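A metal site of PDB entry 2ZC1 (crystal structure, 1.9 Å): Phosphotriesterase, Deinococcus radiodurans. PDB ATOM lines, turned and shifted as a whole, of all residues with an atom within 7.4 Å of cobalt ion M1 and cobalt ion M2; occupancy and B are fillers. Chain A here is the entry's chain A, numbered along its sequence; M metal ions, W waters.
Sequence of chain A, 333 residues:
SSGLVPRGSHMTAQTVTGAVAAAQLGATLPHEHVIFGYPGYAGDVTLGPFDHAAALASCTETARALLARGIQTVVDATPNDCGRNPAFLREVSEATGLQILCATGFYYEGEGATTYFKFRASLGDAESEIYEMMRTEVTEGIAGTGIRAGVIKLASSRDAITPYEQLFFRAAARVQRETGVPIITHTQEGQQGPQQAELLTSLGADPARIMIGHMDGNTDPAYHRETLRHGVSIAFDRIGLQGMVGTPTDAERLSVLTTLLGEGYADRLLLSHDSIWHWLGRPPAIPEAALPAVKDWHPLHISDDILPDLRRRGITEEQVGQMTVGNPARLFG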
ATOM      1  N   HIS A  31      11.005  20.286 -20.190  1.00  0.00           N
ATOM      2  CA  HIS A  31      12.358  19.771 -20.421  1.00  0.00           C
ATOM      3  C   HIS A  31      13.425  20.626 -19.727  1.00  0.00           C
ATOM      4  O   HIS A  31      13.864  21.635 -20.281  1.00  0.00           O
ATOM      5  CB  HIS A  31      12.677  19.720 -21.937  1.00  0.00           C
ATOM      6  CG  HIS A  31      13.962  19.003 -22.256  1.00  0.00           C
ATOM      7  ND1 HIS A  31      14.029  17.965 -23.169  1.00  0.00           N
ATOM      8  CD2 HIS A  31      15.223  19.180 -21.798  1.00  0.00           C
ATOM      9  CE1 HIS A  31      15.277  17.525 -23.249  1.00  0.00           C
ATOM     10  NE2 HIS A  31      16.024  18.251 -22.426  1.00  0.00           N
ATOM     11  N   GLU A  32      13.807  20.227 -18.524  1.00  0.00           N
ATOM     12  CA  GLU A  32      14.858  20.922 -17.770  1.00  0.00           C
ATOM     13  C   GLU A  32      15.706  19.863 -17.068  1.00  0.00           C
ATOM     14  O   GLU A  32      15.381  18.668 -17.067  1.00  0.00           O
ATOM     15  CB  GLU A  32      14.242  21.848 -16.718  1.00  0.00           C
ATOM     16  CG  GLU A  32      13.132  22.779 -17.236  1.00  0.00           C
ATOM     17  CD  GLU A  32      13.651  23.879 -18.126  1.00  0.00           C
ATOM     18  OE1 GLU A  32      14.868  24.195 -18.056  1.00  0.00           O
ATOM     19  OE2 GLU A  32      12.839  24.452 -18.872  1.00  0.00           O
ATOM     20  N   HIS A  33      16.804  20.312 -16.447  1.00  0.00           N
ATOM     21  CA  HIS A  33      17.670  19.404 -15.705  1.00  0.00           C
ATOM     22  C   HIS A  33      18.017  20.015 -14.358  1.00  0.00           C
ATOM     23  O   HIS A  33      18.742  20.990 -14.299  1.00  0.00           O
ATOM     24  CB  HIS A  33      18.963  19.159 -16.498  1.00  0.00           C
ATOM     25  CG  HIS A  33      18.738  18.480 -17.808  1.00  0.00           C
ATOM     26  ND1 HIS A  33      18.457  17.135 -17.899  1.00  0.00           N
ATOM     27  CD2 HIS A  33      18.674  18.970 -19.072  1.00  0.00           C
ATOM     28  CE1 HIS A  33      18.228  16.826 -19.159  1.00  0.00           C
ATOM     29  NE2 HIS A  33      18.336  17.916 -19.884  1.00  0.00           N
ATOM     30  N   PHE A  36      22.860  17.666 -13.710  1.00  0.00           N
ATOM     31  CA  PHE A  36      23.278  17.000 -14.943  1.00  0.00           C
ATOM     32  C   PHE A  36      24.802  16.824 -14.969  1.00  0.00           C
ATOM     33  O   PHE A  36      25.551  17.684 -14.517  1.00  0.00           O
ATOM     34  CB  PHE A  36      22.826  17.841 -16.134  1.00  0.00           C
ATOM     35  CG  PHE A  36      23.133  17.226 -17.476  1.00  0.00           C
ATOM     36  CD1 PHE A  36      24.408  17.326 -18.036  1.00  0.00           C
ATOM     37  CD2 PHE A  36      22.141  16.549 -18.171  1.00  0.00           C
ATOM     38  CE1 PHE A  36      24.695  16.738 -19.277  1.00  0.00           C
ATOM     39  CE2 PHE A  36      22.412  15.958 -19.419  1.00  0.00           C
ATOM     40  CZ  PHE A  36      23.690  16.047 -19.964  1.00  0.00           C
ATOM     41  N   ALA A  77      14.393  15.981 -17.667  1.00  0.00           N
ATOM     42  CA  ALA A  77      14.682  15.113 -18.785  1.00  0.00           C
ATOM     43  C   ALA A  77      16.022  14.398 -18.769  1.00  0.00           C
ATOM     44  O   ALA A  77      16.438  13.846 -19.785  1.00  0.00           O
ATOM     45  CB  ALA A  77      14.526  15.915 -20.020  1.00  0.00           C
ATOM     46  N   THR A  78      16.683  14.370 -17.616  1.00  0.00           N
ATOM     47  CA  THR A  78      18.000  13.775 -17.468  1.00  0.00           C
ATOM     48  C   THR A  78      18.037  12.265 -17.689  1.00  0.00           C
ATOM     49  O   THR A  78      17.402  11.523 -16.954  1.00  0.00           O
ATOM     50  CB  THR A  78      18.576  14.063 -16.061  1.00  0.00           C
ATOM     51  OG1 THR A  78      18.349  15.437 -15.739  1.00  0.00           O
ATOM     52  CG2 THR A  78      20.075  13.737 -15.996  1.00  0.00           C
ATOM     53  N   PRO A  79      18.810  11.798 -18.707  1.00  0.00           N
ATOM     54  CA  PRO A  79      18.982  10.387 -19.060  1.00  0.00           C
ATOM     55  C   PRO A  79      19.668   9.670 -17.908  1.00  0.00           C
ATOM     56  O   PRO A  79      20.401  10.296 -17.133  1.00  0.00           O
ATOM     57  CB  PRO A  79      19.900  10.432 -20.276  1.00  0.00           C
ATOM     58  CG  PRO A  79      19.592  11.723 -20.900  1.00  0.00           C
ATOM     59  CD  PRO A  79      19.434  12.676 -19.715  1.00  0.00           C
ATOM     60  N   TYR A 107      21.151   8.507 -23.151  1.00  0.00           N
ATOM     61  CA  TYR A 107      21.367   9.588 -24.094  1.00  0.00           C
ATOM     62  C   TYR A 107      21.744   9.092 -25.479  1.00  0.00           C
ATOM     63  O   TYR A 107      21.973   7.895 -25.683  1.00  0.00           O
ATOM     64  CB  TYR A 107      22.403  10.596 -23.537  1.00  0.00           C
ATOM     65  CG  TYR A 107      22.094  12.044 -23.885  1.00  0.00           C
ATOM     66  CD1 TYR A 107      20.800  12.430 -24.229  1.00  0.00           C
ATOM     67  CD2 TYR A 107      23.081  13.023 -23.847  1.00  0.00           C
ATOM     68  CE1 TYR A 107      20.495  13.754 -24.522  1.00  0.00           C
ATOM     69  CE2 TYR A 107      22.770  14.371 -24.137  1.00  0.00           C
ATOM     70  CZ  TYR A 107      21.484  14.724 -24.470  1.00  0.00           C
ATOM     71  OH  TYR A 107      21.153  16.045 -24.704  1.00  0.00           O
ATOM     72  N   TYR A 108      21.815  10.005 -26.445  1.00  0.00           N
ATOM     73  CA  TYR A 108      22.142   9.637 -27.815  1.00  0.00           C
ATOM     74  C   TYR A 108      23.591   9.160 -27.935  1.00  0.00           C
ATOM     75  O   TYR A 108      24.418   9.421 -27.063  1.00  0.00           O
ATOM     76  CB  TYR A 108      21.817  10.787 -28.773  1.00  0.00           C
ATOM     77  CG  TYR A 108      22.808  11.923 -28.825  1.00  0.00           C
ATOM     78  CD1 TYR A 108      22.955  12.821 -27.754  1.00  0.00           C
ATOM     79  CD2 TYR A 108      23.602  12.117 -29.956  1.00  0.00           C
ATOM     80  CE1 TYR A 108      23.880  13.892 -27.826  1.00  0.00           C
ATOM     81  CE2 TYR A 108      24.533  13.178 -30.036  1.00  0.00           C
ATOM     82  CZ  TYR A 108      24.657  14.049 -28.974  1.00  0.00           C
ATOM     83  OH  TYR A 108      25.534  15.106 -29.076  1.00  0.00           O
ATOM     84  N   GLU A 111      26.900  11.430 -27.205  1.00  0.00           N
ATOM     85  CA  GLU A 111      27.308  11.893 -25.889  1.00  0.00           C
ATOM     86  C   GLU A 111      26.996  10.953 -24.735  1.00  0.00           C
ATOM     87  O   GLU A 111      27.433  11.199 -23.613  1.00  0.00           O
ATOM     88  CB  GLU A 111      26.666  13.250 -25.570  1.00  0.00           C
ATOM     89  CG  GLU A 111      27.362  14.433 -26.196  1.00  0.00           C
ATOM     90  CD  GLU A 111      26.612  15.742 -25.971  1.00  0.00           C
ATOM     91  OE1 GLU A 111      25.823  15.845 -25.002  1.00  0.00           O
ATOM     92  OE2 GLU A 111      26.819  16.674 -26.762  1.00  0.00           O
ATOM     93  N   KCX A 153      12.751   9.116 -21.832  1.00  0.00           N
ATOM     94  CA  KCX A 153      13.557  10.061 -22.603  1.00  0.00           C
ATOM     95  CB  KCX A 153      14.568  10.786 -21.692  1.00  0.00           C
ATOM     96  CG  KCX A 153      15.673  11.595 -22.397  1.00  0.00           C
ATOM     97  CD  KCX A 153      15.130  12.792 -23.154  1.00  0.00           C
ATOM     98  CE  KCX A 153      16.249  13.635 -23.766  1.00  0.00           C
ATOM     99  NZ  KCX A 153      16.971  14.402 -22.738  1.00  0.00           N
ATOM    100  C   KCX A 153      14.278   9.277 -23.702  1.00  0.00           C
ATOM    101  O   KCX A 153      14.947   8.288 -23.427  1.00  0.00           O
ATOM    102  CX  KCX A 153      17.754  15.464 -22.978  1.00  0.00           C
ATOM    103  OQ1 KCX A 153      17.986  15.866 -24.150  1.00  0.00           O
ATOM    104  OQ2 KCX A 153      18.321  16.068 -22.040  1.00  0.00           O
ATOM    105  N   LEU A 154      14.114   9.722 -24.924  1.00  0.00           N
ATOM    106  CA  LEU A 154      14.758   9.143 -26.084  1.00  0.00           C
ATOM    107  C   LEU A 154      15.620  10.226 -26.710  1.00  0.00           C
ATOM    108  O   LEU A 154      15.316  11.415 -26.577  1.00  0.00           O
ATOM    109  CB  LEU A 154      13.700   8.711 -27.115  1.00  0.00           C
ATOM    110  CG  LEU A 154      12.829   7.515 -26.727  1.00  0.00           C
ATOM    111  CD1 LEU A 154      11.826   7.233 -27.854  1.00  0.00           C
ATOM    112  CD2 LEU A 154      13.729   6.289 -26.510  1.00  0.00           C
ATOM    113  N   ALA A 155      16.662   9.814 -27.435  1.00  0.00           N
ATOM    114  CA  ALA A 155      17.546  10.781 -28.075  1.00  0.00           C
ATOM    115  C   ALA A 155      18.224  10.186 -29.289  1.00  0.00           C
ATOM    116  O   ALA A 155      18.638   9.042 -29.273  1.00  0.00           O
ATOM    117  CB  ALA A 155      18.611  11.246 -27.079  1.00  0.00           C
ATOM    118  N   THR A 185      11.735  13.652 -26.351  1.00  0.00           N
ATOM    119  CA  THR A 185      12.965  13.331 -27.009  1.00  0.00           C
ATOM    120  C   THR A 185      13.950  14.473 -27.234  1.00  0.00           C
ATOM    121  O   THR A 185      13.610  15.644 -27.143  1.00  0.00           O
ATOM    122  CB  THR A 185      12.695  12.720 -28.412  1.00  0.00           C
ATOM    123  OG1 THR A 185      12.496  13.785 -29.358  1.00  0.00           O
ATOM    124  CG2 THR A 185      11.437  11.840 -28.389  1.00  0.00           C
ATOM    125  N   HIS A 186      15.157  14.064 -27.556  1.00  0.00           N
ATOM    126  CA  HIS A 186      16.245  14.948 -27.919  1.00  0.00           C
ATOM    127  C   HIS A 186      16.484  14.732 -29.417  1.00  0.00           C
ATOM    128  O   HIS A 186      16.513  13.581 -29.875  1.00  0.00           O
ATOM    129  CB  HIS A 186      17.510  14.546 -27.145  1.00  0.00           C
ATOM    130  CG  HIS A 186      18.794  14.988 -27.799  1.00  0.00           C
ATOM    131  ND1 HIS A 186      19.617  15.939 -27.230  1.00  0.00           N
ATOM    132  CD2 HIS A 186      19.428  14.559 -28.915  1.00  0.00           C
ATOM    133  CE1 HIS A 186      20.714  16.062 -27.964  1.00  0.00           C
ATOM    134  NE2 HIS A 186      20.623  15.235 -28.994  1.00  0.00           N
ATOM    135  N   THR A 187      16.600  15.809 -30.181  1.00  0.00           N
ATOM    136  CA  THR A 187      16.983  15.699 -31.578  1.00  0.00           C
ATOM    137  C   THR A 187      18.283  16.486 -31.617  1.00  0.00           C
ATOM    138  O   THR A 187      18.427  17.524 -30.941  1.00  0.00           O
ATOM    139  CB  THR A 187      15.999  16.365 -32.579  1.00  0.00           C
ATOM    140  OG1 THR A 187      15.773  17.732 -32.211  1.00  0.00           O
ATOM    141  CG2 THR A 187      14.683  15.571 -32.642  1.00  0.00           C
ATOM    142  N   GLN A 188      19.231  15.990 -32.393  1.00  0.00           N
ATOM    143  CA  GLN A 188      20.538  16.621 -32.495  1.00  0.00           C
ATOM    144  C   GLN A 188      20.690  17.588 -33.665  1.00  0.00           C
ATOM    145  O   GLN A 188      20.465  17.229 -34.812  1.00  0.00           O
ATOM    146  CB  GLN A 188      21.603  15.530 -32.568  1.00  0.00           C
ATOM    147  CG  GLN A 188      23.017  16.029 -32.639  1.00  0.00           C
ATOM    148  CD  GLN A 188      23.503  16.680 -31.360  1.00  0.00           C
ATOM    149  OE1 GLN A 188      24.492  17.422 -31.376  1.00  0.00           O
ATOM    150  NE2 GLN A 188      22.829  16.391 -30.245  1.00  0.00           N
ATOM    151  N   GLY A 213      11.558  16.765 -29.109  1.00  0.00           N
ATOM    152  CA  GLY A 213      12.230  17.956 -28.615  1.00  0.00           C
ATOM    153  C   GLY A 213      13.339  18.566 -29.441  1.00  0.00           C
ATOM    154  O   GLY A 213      13.675  18.106 -30.542  1.00  0.00           O
ATOM    155  N   HIS A 214      13.912  19.630 -28.863  1.00  0.00           N
ATOM    156  CA  HIS A 214      14.982  20.432 -29.474  1.00  0.00           C
ATOM    157  C   HIS A 214      14.607  20.814 -30.897  1.00  0.00           C
ATOM    158  O   HIS A 214      15.466  20.946 -31.769  1.00  0.00           O
ATOM    159  CB  HIS A 214      16.310  19.683 -29.487  1.00  0.00           C
ATOM    160  CG  HIS A 214      16.760  19.206 -28.137  1.00  0.00           C
ATOM    161  ND1 HIS A 214      16.229  19.673 -26.954  1.00  0.00           N
ATOM    162  CD2 HIS A 214      17.683  18.274 -27.794  1.00  0.00           C
ATOM    163  CE1 HIS A 214      16.813  19.057 -25.941  1.00  0.00           C
ATOM    164  NE2 HIS A 214      17.693  18.200 -26.425  1.00  0.00           N
ATOM    165  N   ASP A 237      12.535  23.665 -26.777  1.00  0.00           N
ATOM    166  CA  ASP A 237      12.968  23.478 -25.411  1.00  0.00           C
ATOM    167  C   ASP A 237      14.367  23.855 -24.973  1.00  0.00           C
ATOM    168  O   ASP A 237      14.809  23.403 -23.932  1.00  0.00           O
ATOM    169  CB  ASP A 237      12.687  22.028 -24.991  1.00  0.00           C
ATOM    170  CG  ASP A 237      13.269  21.018 -25.953  1.00  0.00           C
ATOM    171  OD1 ASP A 237      14.270  21.363 -26.634  1.00  0.00           O
ATOM    172  OD2 ASP A 237      12.757  19.870 -26.037  1.00  0.00           O
ATOM    173  N   ARG A 238      15.063  24.671 -25.766  1.00  0.00           N
ATOM    174  CA  ARG A 238      16.392  25.139 -25.393  1.00  0.00           C
ATOM    175  C   ARG A 238      16.375  26.669 -25.526  1.00  0.00           C
ATOM    176  O   ARG A 238      17.370  27.281 -25.958  1.00  0.00           O
ATOM    177  CB  ARG A 238      17.453  24.574 -26.323  1.00  0.00           C
ATOM    178  CG  ARG A 238      17.251  23.087 -26.601  1.00  0.00           C
ATOM    179  CD  ARG A 238      18.415  22.521 -27.343  1.00  0.00           C
ATOM    180  NE  ARG A 238      19.462  22.129 -26.409  1.00  0.00           N
ATOM    181  CZ  ARG A 238      20.762  22.239 -26.643  1.00  0.00           C
ATOM    182  NH1 ARG A 238      21.195  22.751 -27.800  1.00  0.00           N
ATOM    183  NH2 ARG A 238      21.634  21.811 -25.732  1.00  0.00           N
ATOM    184  N   HIS A 273      13.594  25.376 -21.445  1.00  0.00           N
ATOM    185  CA  HIS A 273      14.935  25.937 -21.559  1.00  0.00           C
ATOM    186  C   HIS A 273      16.076  24.945 -21.648  1.00  0.00           C
ATOM    187  O   HIS A 273      17.149  25.321 -22.104  1.00  0.00           O
ATOM    188  CB  HIS A 273      15.265  26.828 -20.332  1.00  0.00           C
ATOM    189  CG  HIS A 273      14.117  27.657 -19.828  1.00  0.00           C
ATOM    190  ND1 HIS A 273      13.991  28.988 -20.119  1.00  0.00           N
ATOM    191  CD2 HIS A 273      13.078  27.339 -19.022  1.00  0.00           C
ATOM    192  CE1 HIS A 273      12.913  29.472 -19.523  1.00  0.00           C
ATOM    193  NE2 HIS A 273      12.343  28.488 -18.850  1.00  0.00           N
ATOM    194  N   ASP A 274      15.856  23.712 -21.177  1.00  0.00           N
ATOM    195  CA  ASP A 274      16.920  22.712 -21.165  1.00  0.00           C
ATOM    196  C   ASP A 274      18.009  23.268 -20.237  1.00  0.00           C
ATOM    197  O   ASP A 274      19.192  23.076 -20.472  1.00  0.00           O
ATOM    198  CB  ASP A 274      17.480  22.495 -22.583  1.00  0.00           C
ATOM    199  CG  ASP A 274      18.288  21.224 -22.712  1.00  0.00           C
ATOM    200  OD1 ASP A 274      18.160  20.353 -21.827  1.00  0.00           O
ATOM    201  OD2 ASP A 274      19.057  21.067 -23.680  1.00  0.00           O
ATOM    202  N   SER A 275      17.598  23.940 -19.179  1.00  0.00           N
ATOM    203  CA  SER A 275      18.560  24.507 -18.235  1.00  0.00           C
ATOM    204  C   SER A 275      19.173  23.428 -17.349  1.00  0.00           C
ATOM    205  O   SER A 275      18.645  22.313 -17.227  1.00  0.00           O
ATOM    206  CB  SER A 275      17.850  25.554 -17.353  1.00  0.00           C
ATOM    207  OG  SER A 275      16.928  24.938 -16.478  1.00  0.00           O
ATOM    208  N   ILE A 276      20.319  23.727 -16.757  1.00  0.00           N
ATOM    209  CA  ILE A 276      20.925  22.789 -15.812  1.00  0.00           C
ATOM    210  C   ILE A 276      21.069  23.613 -14.543  1.00  0.00           C
ATOM    211  O   ILE A 276      21.811  24.602 -14.513  1.00  0.00           O
ATOM    212  CB  ILE A 276      22.282  22.272 -16.323  1.00  0.00           C
ATOM    213  CG1 ILE A 276      22.037  21.276 -17.482  1.00  0.00           C
ATOM    214  CG2 ILE A 276      23.060  21.580 -15.184  1.00  0.00           C
ATOM    215  CD1 ILE A 276      23.282  20.918 -18.269  1.00  0.00           C
HETATM  216 CO    CO M   1      19.233  17.067 -25.267  1.00  0.00          CO
HETATM  217 CO    CO M   2      18.205  18.123 -22.025  1.00  0.00          CO
HETATM  218  O   HOH W   1      21.377  17.994 -21.962  1.00  0.00           O
HETATM  219  O   HOH W   2      19.271  18.411 -23.588  1.00  0.00           O
HETATM  220  O   HOH W   3      20.699  18.655 -26.139  1.00  0.00           O
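O of Ala 77 sits at hydrogen-bond distance from NZ of KCX 153.
ND1 of His 33 is in hydrogen-bond range of OG1 of Thr 78 (2.7 Å).
The backbone NH (N) of His 33 lies within hydrogen-bond range of the backbone carbonyl oxygen (O) of Ser 275, at 2.8 Å.
The side-chain hydroxyl (OG1) of Thr 187 is in hydrogen-bond range of the backbone carbonyl oxygen (O) of His 214.
OD1 of Asp 237 sits at hydrogen-bond distance from ND1 of His 214 (2.6 Å).
OD2 of Asp 274 is in salt-bridge range of NE of Arg 238 (3.0 Å).
The side-chain amide nitrogen (NE2) of Gln 188 sits at hydrogen-bond distance from a ring nitrogen (NE2) of His 186.
N of His 186 is in hydrogen-bond range of O of Leu 154.
Of the 25 residues printed, 4 come within 4 Å of cobalt ion M1.
The nearest printed residue that does not touch cobalt ion M2 is His 214 (4.3 Å).
Cobalt ion M1 is bound by OQ1 of KCX 153, at 2.1 Å.
Cobalt ion M1 is bound by water W2, 2.2 Å away.
NE2 of His 214 binds cobalt ion M1, at 2.2 Å.
OH of Tyr 107 is bound to cobalt ion M1 (2.2 Å).
ND1 of His 186 is bound to cobalt ion M1 (2.3 Å).
Water W3 binds cobalt ion M1.
Cobalt ion M1 has six donor atoms within binding distance.
Cobalt ion M2 is bound by water W2 (1.9 Å).
OQ2 of KCX 153 binds cobalt ion M2 (2.1 Å).
NE2 of His 33 is bound to cobalt ion M2 (2.2 Å).
NE2 of His 31 is bound to cobalt ion M2 (2.2 Å).
The side-chain carboxylate (OD1) of Asp 274 is bound to cobalt ion M2 (2.2 Å).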
